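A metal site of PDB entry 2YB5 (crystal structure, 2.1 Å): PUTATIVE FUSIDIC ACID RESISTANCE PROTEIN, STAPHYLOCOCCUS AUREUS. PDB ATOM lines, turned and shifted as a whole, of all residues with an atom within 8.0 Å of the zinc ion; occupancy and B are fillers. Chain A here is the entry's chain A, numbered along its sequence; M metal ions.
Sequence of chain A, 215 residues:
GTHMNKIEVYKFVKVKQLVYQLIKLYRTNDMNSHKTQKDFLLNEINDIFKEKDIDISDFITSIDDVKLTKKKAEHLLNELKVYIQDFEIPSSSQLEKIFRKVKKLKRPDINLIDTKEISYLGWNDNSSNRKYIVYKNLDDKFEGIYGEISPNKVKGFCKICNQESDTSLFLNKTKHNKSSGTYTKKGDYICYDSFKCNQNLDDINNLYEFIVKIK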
ATOM      1  N   TYR A 120      23.307   9.899  22.222  1.00  0.00           N
ATOM      2  CA  TYR A 120      22.569  11.148  22.246  1.00  0.00           C
ATOM      3  C   TYR A 120      21.234  11.002  21.510  1.00  0.00           C
ATOM      4  O   TYR A 120      21.104  10.196  20.590  1.00  0.00           O
ATOM      5  CB  TYR A 120      23.408  12.269  21.637  1.00  0.00           C
ATOM      6  CG  TYR A 120      23.533  12.265  20.143  1.00  0.00           C
ATOM      7  CD1 TYR A 120      22.583  12.895  19.336  1.00  0.00           C
ATOM      8  CD2 TYR A 120      24.652  11.690  19.517  1.00  0.00           C
ATOM      9  CE1 TYR A 120      22.721  12.911  17.946  1.00  0.00           C
ATOM     10  CE2 TYR A 120      24.782  11.695  18.158  1.00  0.00           C
ATOM     11  CZ  TYR A 120      23.828  12.319  17.368  1.00  0.00           C
ATOM     12  OH  TYR A 120      23.985  12.343  16.003  1.00  0.00           O
ATOM     13  N   GLY A 156      28.737  12.273   2.616  1.00  0.00           N
ATOM     14  CA  GLY A 156      29.986  12.815   3.145  1.00  0.00           C
ATOM     15  C   GLY A 156      30.300  12.304   4.529  1.00  0.00           C
ATOM     16  O   GLY A 156      29.637  11.386   5.024  1.00  0.00           O
ATOM     17  N   PHE A 157      31.297  12.911   5.179  1.00  0.00           N
ATOM     18  CA  PHE A 157      31.700  12.520   6.519  1.00  0.00           C
ATOM     19  C   PHE A 157      30.882  13.306   7.514  1.00  0.00           C
ATOM     20  O   PHE A 157      30.920  14.538   7.504  1.00  0.00           O
ATOM     21  CB  PHE A 157      33.163  12.837   6.793  1.00  0.00           C
ATOM     22  CG  PHE A 157      34.114  12.261   5.808  1.00  0.00           C
ATOM     23  CD1 PHE A 157      34.286  10.886   5.716  1.00  0.00           C
ATOM     24  CD2 PHE A 157      34.868  13.093   4.985  1.00  0.00           C
ATOM     25  CE1 PHE A 157      35.184  10.352   4.816  1.00  0.00           C
ATOM     26  CE2 PHE A 157      35.763  12.568   4.080  1.00  0.00           C
ATOM     27  CZ  PHE A 157      35.918  11.177   3.990  1.00  0.00           C
ATOM     28  N   CYS A 158      30.159  12.598   8.376  1.00  0.00           N
ATOM     29  CA  CYS A 158      29.444  13.239   9.475  1.00  0.00           C
ATOM     30  C   CYS A 158      30.473  13.783  10.461  1.00  0.00           C
ATOM     31  O   CYS A 158      31.345  13.061  10.891  1.00  0.00           O
ATOM     32  CB  CYS A 158      28.542  12.236  10.186  1.00  0.00           C
ATOM     33  SG  CYS A 158      27.934  12.763  11.821  1.00  0.00           S
ATOM     34  N   LYS A 159      30.358  15.050  10.848  1.00  0.00           N
ATOM     35  CA  LYS A 159      31.329  15.587  11.793  1.00  0.00           C
ATOM     36  C   LYS A 159      31.074  15.249  13.269  1.00  0.00           C
ATOM     37  O   LYS A 159      31.799  15.736  14.140  1.00  0.00           O
ATOM     38  CB  LYS A 159      31.504  17.093  11.580  1.00  0.00           C
ATOM     39  CG  LYS A 159      32.028  17.418  10.174  1.00  0.00           C
ATOM     40  CD  LYS A 159      33.437  16.865   9.898  1.00  0.00           C
ATOM     41  CE  LYS A 159      33.873  17.140   8.461  1.00  0.00           C
ATOM     42  NZ  LYS A 159      35.212  16.556   8.127  1.00  0.00           N
ATOM     43  N   ILE A 160      30.093  14.391  13.562  1.00  0.00           N
ATOM     44  CA  ILE A 160      29.942  13.844  14.907  1.00  0.00           C
ATOM     45  C   ILE A 160      30.595  12.461  15.017  1.00  0.00           C
ATOM     46  O   ILE A 160      31.475  12.264  15.852  1.00  0.00           O
ATOM     47  CB  ILE A 160      28.479  13.771  15.319  1.00  0.00           C
ATOM     48  CG1 ILE A 160      27.945  15.186  15.574  1.00  0.00           C
ATOM     49  CG2 ILE A 160      28.309  12.919  16.584  1.00  0.00           C
ATOM     50  CD1 ILE A 160      26.471  15.272  15.614  1.00  0.00           C
ATOM     51  N   CYS A 161      30.181  11.517  14.189  1.00  0.00           N
ATOM     52  CA  CYS A 161      30.665  10.159  14.268  1.00  0.00           C
ATOM     53  C   CYS A 161      31.867   9.916  13.359  1.00  0.00           C
ATOM     54  O   CYS A 161      32.479   8.864  13.431  1.00  0.00           O
ATOM     55  CB  CYS A 161      29.541   9.169  13.906  1.00  0.00           C
ATOM     56  SG  CYS A 161      28.939   9.283  12.197  1.00  0.00           S
ATOM     57  N   ASN A 162      32.176  10.904  12.512  1.00  0.00           N
ATOM     58  CA  ASN A 162      33.303  10.866  11.575  1.00  0.00           C
ATOM     59  C   ASN A 162      33.216   9.821  10.462  1.00  0.00           C
ATOM     60  O   ASN A 162      34.175   9.649   9.728  1.00  0.00           O
ATOM     61  CB  ASN A 162      34.636  10.719  12.314  1.00  0.00           C
ATOM     62  CG  ASN A 162      34.975  11.931  13.149  1.00  0.00           C
ATOM     63  OD1 ASN A 162      35.498  11.810  14.267  1.00  0.00           O
ATOM     64  ND2 ASN A 162      34.708  13.113  12.620  1.00  0.00           N
ATOM     65  N   GLN A 163      32.080   9.145  10.300  1.00  0.00           N
ATOM     66  CA  GLN A 163      31.931   8.182   9.214  1.00  0.00           C
ATOM     67  C   GLN A 163      31.190   8.780   8.019  1.00  0.00           C
ATOM     68  O   GLN A 163      30.617   9.874   8.102  1.00  0.00           O
ATOM     69  CB  GLN A 163      31.237   6.915   9.717  1.00  0.00           C
ATOM     70  CG  GLN A 163      32.018   6.254  10.868  1.00  0.00           C
ATOM     71  CD  GLN A 163      31.673   4.790  11.089  1.00  0.00           C
ATOM     72  OE1 GLN A 163      31.322   4.079  10.157  1.00  0.00           O
ATOM     73  NE2 GLN A 163      31.782   4.348  12.343  1.00  0.00           N
ATOM     74  N   GLU A 164      31.194   8.060   6.897  1.00  0.00           N
ATOM     75  CA  GLU A 164      30.486   8.490   5.694  1.00  0.00           C
ATOM     76  C   GLU A 164      29.021   8.115   5.844  1.00  0.00           C
ATOM     77  O   GLU A 164      28.702   6.992   6.241  1.00  0.00           O
ATOM     78  CB  GLU A 164      31.097   7.848   4.433  1.00  0.00           C
ATOM     79  CG  GLU A 164      30.863   8.662   3.174  1.00  0.00           C
ATOM     80  CD  GLU A 164      31.409   8.002   1.903  1.00  0.00           C
ATOM     81  OE1 GLU A 164      31.424   6.755   1.814  1.00  0.00           O
ATOM     82  OE2 GLU A 164      31.807   8.740   0.977  1.00  0.00           O
ATOM     83  N   SER A 165      28.124   9.062   5.562  1.00  0.00           N
ATOM     84  CA  SER A 165      26.688   8.831   5.669  1.00  0.00           C
ATOM     85  C   SER A 165      25.893   9.814   4.810  1.00  0.00           C
ATOM     86  O   SER A 165      26.482  10.664   4.136  1.00  0.00           O
ATOM     87  CB  SER A 165      26.235   8.936   7.129  1.00  0.00           C
ATOM     88  OG  SER A 165      26.001  10.279   7.503  1.00  0.00           O
ATOM     89  N   ASP A 166      24.570   9.685   4.841  1.00  0.00           N
ATOM     90  CA  ASP A 166      23.701  10.684   4.227  1.00  0.00           C
ATOM     91  C   ASP A 166      23.652  11.854   5.196  1.00  0.00           C
ATOM     92  O   ASP A 166      23.071  11.743   6.281  1.00  0.00           O
ATOM     93  CB  ASP A 166      22.301  10.124   3.982  1.00  0.00           C
ATOM     94  CG  ASP A 166      22.294   8.993   2.945  1.00  0.00           C
ATOM     95  OD1 ASP A 166      23.054   9.058   1.960  1.00  0.00           O
ATOM     96  OD2 ASP A 166      21.508   8.042   3.125  1.00  0.00           O
ATOM     97  N   THR A 167      24.288  12.961   4.824  1.00  0.00           N
ATOM     98  CA  THR A 167      24.492  14.089   5.718  1.00  0.00           C
ATOM     99  C   THR A 167      23.735  15.333   5.253  1.00  0.00           C
ATOM    100  O   THR A 167      23.343  15.441   4.098  1.00  0.00           O
ATOM    101  CB  THR A 167      25.989  14.443   5.843  1.00  0.00           C
ATOM    102  OG1 THR A 167      26.424  15.107   4.655  1.00  0.00           O
ATOM    103  CG2 THR A 167      26.836  13.181   6.072  1.00  0.00           C
ATOM    104  N   TYR A 189      28.281  19.564   8.590  1.00  0.00           N
ATOM    105  CA  TYR A 189      27.546  18.429   8.047  1.00  0.00           C
ATOM    106  C   TYR A 189      27.547  17.252   9.030  1.00  0.00           C
ATOM    107  O   TYR A 189      28.589  16.830   9.505  1.00  0.00           O
ATOM    108  CB  TYR A 189      28.115  18.004   6.682  1.00  0.00           C
ATOM    109  CG  TYR A 189      27.724  18.988   5.566  1.00  0.00           C
ATOM    110  CD1 TYR A 189      28.460  20.145   5.340  1.00  0.00           C
ATOM    111  CD2 TYR A 189      26.595  18.758   4.780  1.00  0.00           C
ATOM    112  CE1 TYR A 189      28.098  21.041   4.338  1.00  0.00           C
ATOM    113  CE2 TYR A 189      26.230  19.663   3.773  1.00  0.00           C
ATOM    114  CZ  TYR A 189      26.977  20.799   3.568  1.00  0.00           C
ATOM    115  OH  TYR A 189      26.609  21.685   2.573  1.00  0.00           O
ATOM    116  N   ILE A 190      26.345  16.751   9.316  1.00  0.00           N
ATOM    117  CA  ILE A 190      26.147  15.612  10.198  1.00  0.00           C
ATOM    118  C   ILE A 190      25.109  14.644   9.612  1.00  0.00           C
ATOM    119  O   ILE A 190      24.380  14.984   8.680  1.00  0.00           O
ATOM    120  CB  ILE A 190      25.680  16.040  11.605  1.00  0.00           C
ATOM    121  CG1 ILE A 190      24.321  16.764  11.533  1.00  0.00           C
ATOM    122  CG2 ILE A 190      26.743  16.911  12.288  1.00  0.00           C
ATOM    123  CD1 ILE A 190      23.756  17.181  12.901  1.00  0.00           C
ATOM    124  N   CYS A 191      25.052  13.444  10.198  1.00  0.00           N
ATOM    125  CA  CYS A 191      24.092  12.425   9.788  1.00  0.00           C
ATOM    126  C   CYS A 191      22.689  13.019   9.873  1.00  0.00           C
ATOM    127  O   CYS A 191      22.294  13.563  10.899  1.00  0.00           O
ATOM    128  CB  CYS A 191      24.199  11.199  10.678  1.00  0.00           C
ATOM    129  SG  CYS A 191      25.787  10.231  10.643  1.00  0.00           S
ATOM    130  N   TYR A 192      21.936  12.931   8.779  1.00  0.00           N
ATOM    131  CA  TYR A 192      20.549  13.351   8.806  1.00  0.00           C
ATOM    132  C   TYR A 192      19.761  12.548   9.845  1.00  0.00           C
ATOM    133  O   TYR A 192      18.946  13.088  10.592  1.00  0.00           O
ATOM    134  CB  TYR A 192      19.895  13.152   7.445  1.00  0.00           C
ATOM    135  CG  TYR A 192      18.543  13.800   7.379  1.00  0.00           C
ATOM    136  CD1 TYR A 192      18.433  15.185   7.295  1.00  0.00           C
ATOM    137  CD2 TYR A 192      17.366  13.052   7.446  1.00  0.00           C
ATOM    138  CE1 TYR A 192      17.197  15.811   7.261  1.00  0.00           C
ATOM    139  CE2 TYR A 192      16.131  13.664   7.407  1.00  0.00           C
ATOM    140  CZ  TYR A 192      16.054  15.052   7.325  1.00  0.00           C
ATOM    141  OH  TYR A 192      14.848  15.702   7.268  1.00  0.00           O
ATOM    142  N   ASP A 193      20.027  11.242   9.868  1.00  0.00           N
ATOM    143  CA  ASP A 193      19.397  10.306  10.790  1.00  0.00           C
ATOM    144  C   ASP A 193      20.327  10.053  11.987  1.00  0.00           C
ATOM    145  O   ASP A 193      21.313   9.332  11.880  1.00  0.00           O
ATOM    146  CB  ASP A 193      19.118   9.000  10.029  1.00  0.00           C
ATOM    147  CG  ASP A 193      18.546   7.925  10.910  1.00  0.00           C
ATOM    148  OD1 ASP A 193      18.236   8.188  12.090  1.00  0.00           O
ATOM    149  OD2 ASP A 193      18.395   6.797  10.417  1.00  0.00           O
ATOM    150  N   SER A 194      20.002  10.665  13.123  1.00  0.00           N
ATOM    151  CA  SER A 194      20.829  10.584  14.319  1.00  0.00           C
ATOM    152  C   SER A 194      20.869   9.171  14.897  1.00  0.00           C
ATOM    153  O   SER A 194      21.822   8.826  15.609  1.00  0.00           O
ATOM    154  CB  SER A 194      20.315  11.574  15.368  1.00  0.00           C
ATOM    155  OG  SER A 194      20.391  12.895  14.872  1.00  0.00           O
ATOM    156  N   PHE A 195      19.883   8.341  14.584  1.00  0.00           N
ATOM    157  CA  PHE A 195      19.887   6.954  15.050  1.00  0.00           C
ATOM    158  C   PHE A 195      20.948   6.141  14.340  1.00  0.00           C
ATOM    159  O   PHE A 195      21.652   5.344  14.974  1.00  0.00           O
ATOM    160  CB  PHE A 195      18.479   6.362  14.968  1.00  0.00           C
ATOM    161  CG  PHE A 195      17.494   7.107  15.816  1.00  0.00           C
ATOM    162  CD1 PHE A 195      17.386   6.824  17.164  1.00  0.00           C
ATOM    163  CD2 PHE A 195      16.777   8.178  15.300  1.00  0.00           C
ATOM    164  CE1 PHE A 195      16.512   7.547  17.973  1.00  0.00           C
ATOM    165  CE2 PHE A 195      15.918   8.913  16.098  1.00  0.00           C
ATOM    166  CZ  PHE A 195      15.784   8.598  17.447  1.00  0.00           C
ATOM    167  N   LYS A 196      21.118   6.362  13.035  1.00  0.00           N
ATOM    168  CA  LYS A 196      22.236   5.762  12.306  1.00  0.00           C
ATOM    169  C   LYS A 196      23.578   6.282  12.836  1.00  0.00           C
ATOM    170  O   LYS A 196      24.504   5.493  13.055  1.00  0.00           O
ATOM    171  CB  LYS A 196      22.113   6.063  10.818  1.00  0.00           C
ATOM    172  CG  LYS A 196      23.169   5.360   9.951  1.00  0.00           C
ATOM    173  CD  LYS A 196      23.354   6.052   8.608  1.00  0.00           C
ATOM    174  CE  LYS A 196      24.401   5.320   7.760  1.00  0.00           C
ATOM    175  NZ  LYS A 196      24.769   6.048   6.516  1.00  0.00           N
ATOM    176  N   CYS A 197      23.682   7.598  13.022  1.00  0.00           N
ATOM    177  CA  CYS A 197      24.835   8.242  13.670  1.00  0.00           C
ATOM    178  C   CYS A 197      25.237   7.558  14.989  1.00  0.00           C
ATOM    179  O   CYS A 197      26.421   7.261  15.214  1.00  0.00           O
ATOM    180  CB  CYS A 197      24.527   9.712  13.978  1.00  0.00           C
ATOM    181  SG  CYS A 197      25.957  10.704  14.462  1.00  0.00           S
ATOM    182  N   ASN A 198      24.247   7.316  15.840  1.00  0.00           N
ATOM    183  CA  ASN A 198      24.488   6.704  17.146  1.00  0.00           C
ATOM    184  C   ASN A 198      24.976   5.248  17.092  1.00  0.00           C
ATOM    185  O   ASN A 198      25.619   4.790  18.019  1.00  0.00           O
ATOM    186  CB  ASN A 198      23.241   6.796  18.024  1.00  0.00           C
ATOM    187  CG  ASN A 198      23.155   8.118  18.750  1.00  0.00           C
ATOM    188  OD1 ASN A 198      23.777   8.288  19.805  1.00  0.00           O
ATOM    189  ND2 ASN A 198      22.396   9.075  18.203  1.00  0.00           N
ATOM    190  N   GLN A 199      24.692   4.560  15.977  1.00  0.00           N
ATOM    191  CA  GLN A 199      25.270   3.241  15.692  1.00  0.00           C
ATOM    192  C   GLN A 199      26.763   3.347  15.347  1.00  0.00           C
ATOM    193  O   GLN A 199      27.511   2.397  15.550  1.00  0.00           O
ATOM    194  CB  GLN A 199      24.536   2.528  14.552  1.00  0.00           C
ATOM    195  CG  GLN A 199      23.069   2.191  14.833  1.00  0.00           C
ATOM    196  CD  GLN A 199      22.906   1.139  15.917  1.00  0.00           C
ATOM    197  OE1 GLN A 199      23.310   1.359  17.058  1.00  0.00           O
ATOM    198  NE2 GLN A 199      22.317  -0.005  15.555  1.00  0.00           N
ATOM    199  N   ASN A 200      27.178   4.488  14.810  1.00  0.00           N
ATOM    200  CA  ASN A 200      28.565   4.723  14.430  1.00  0.00           C
ATOM    201  C   ASN A 200      29.401   5.398  15.531  1.00  0.00           C
ATOM    202  O   ASN A 200      30.628   5.343  15.488  1.00  0.00           O
ATOM    203  CB  ASN A 200      28.644   5.633  13.190  1.00  0.00           C
ATOM    204  CG  ASN A 200      27.749   5.160  12.047  1.00  0.00           C
ATOM    205  OD1 ASN A 200      27.413   3.974  11.929  1.00  0.00           O
ATOM    206  ND2 ASN A 200      27.347   6.115  11.175  1.00  0.00           N
ATOM    207  N   LEU A 201      28.746   6.078  16.463  1.00  0.00           N
ATOM    208  CA  LEU A 201      29.464   6.970  17.375  1.00  0.00           C
ATOM    209  C   LEU A 201      30.189   6.179  18.473  1.00  0.00           C
ATOM    210  O   LEU A 201      29.554   5.612  19.361  1.00  0.00           O
ATOM    211  CB  LEU A 201      28.503   7.984  18.003  1.00  0.00           C
ATOM    212  CG  LEU A 201      29.094   8.961  19.028  1.00  0.00           C
ATOM    213  CD1 LEU A 201      30.243   9.776  18.433  1.00  0.00           C
ATOM    214  CD2 LEU A 201      27.984   9.882  19.583  1.00  0.00           C
HETATM  215 ZN    ZN M   1      27.046  10.711  12.292  1.00  0.00          ZN
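The backbone NH of Ile 160 lies close to the side-chain sulfur of Cys 158 (3.2 Å). The side-chain hydroxyl of Ser 165 sits close to the side-chain sulfur of Cys 191 (3.1 Å). The side-chain amide nitrogen (ND2) of Asn 200 lies close to the side-chain sulfur (SG) of Cys 161 (3.7 Å). SG of Cys 161 lies close to N of Gln 163 (3.7 Å). The side-chain hydroxyl of Tyr 120 lies close to the side-chain sulfur of Cys 197. The backbone carbonyl oxygen of Gln 163 lies within hydrogen-bond range of the backbone NH of Cys 158 (2.8 Å).
Within 4 Å of the zinc ion: Cys 158, Cys 161, Cys 191 and Cys 197.
The zinc ion is bound by the side-chain sulfur (SG) of Cys 191 (2.1 Å), the side-chain sulfur (SG) of Cys 158 (2.3 Å), the side-chain sulfur (SG) of Cys 161 (2.4 Å) and the side-chain sulfur (SG) of Cys 197 (2.4 Å).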
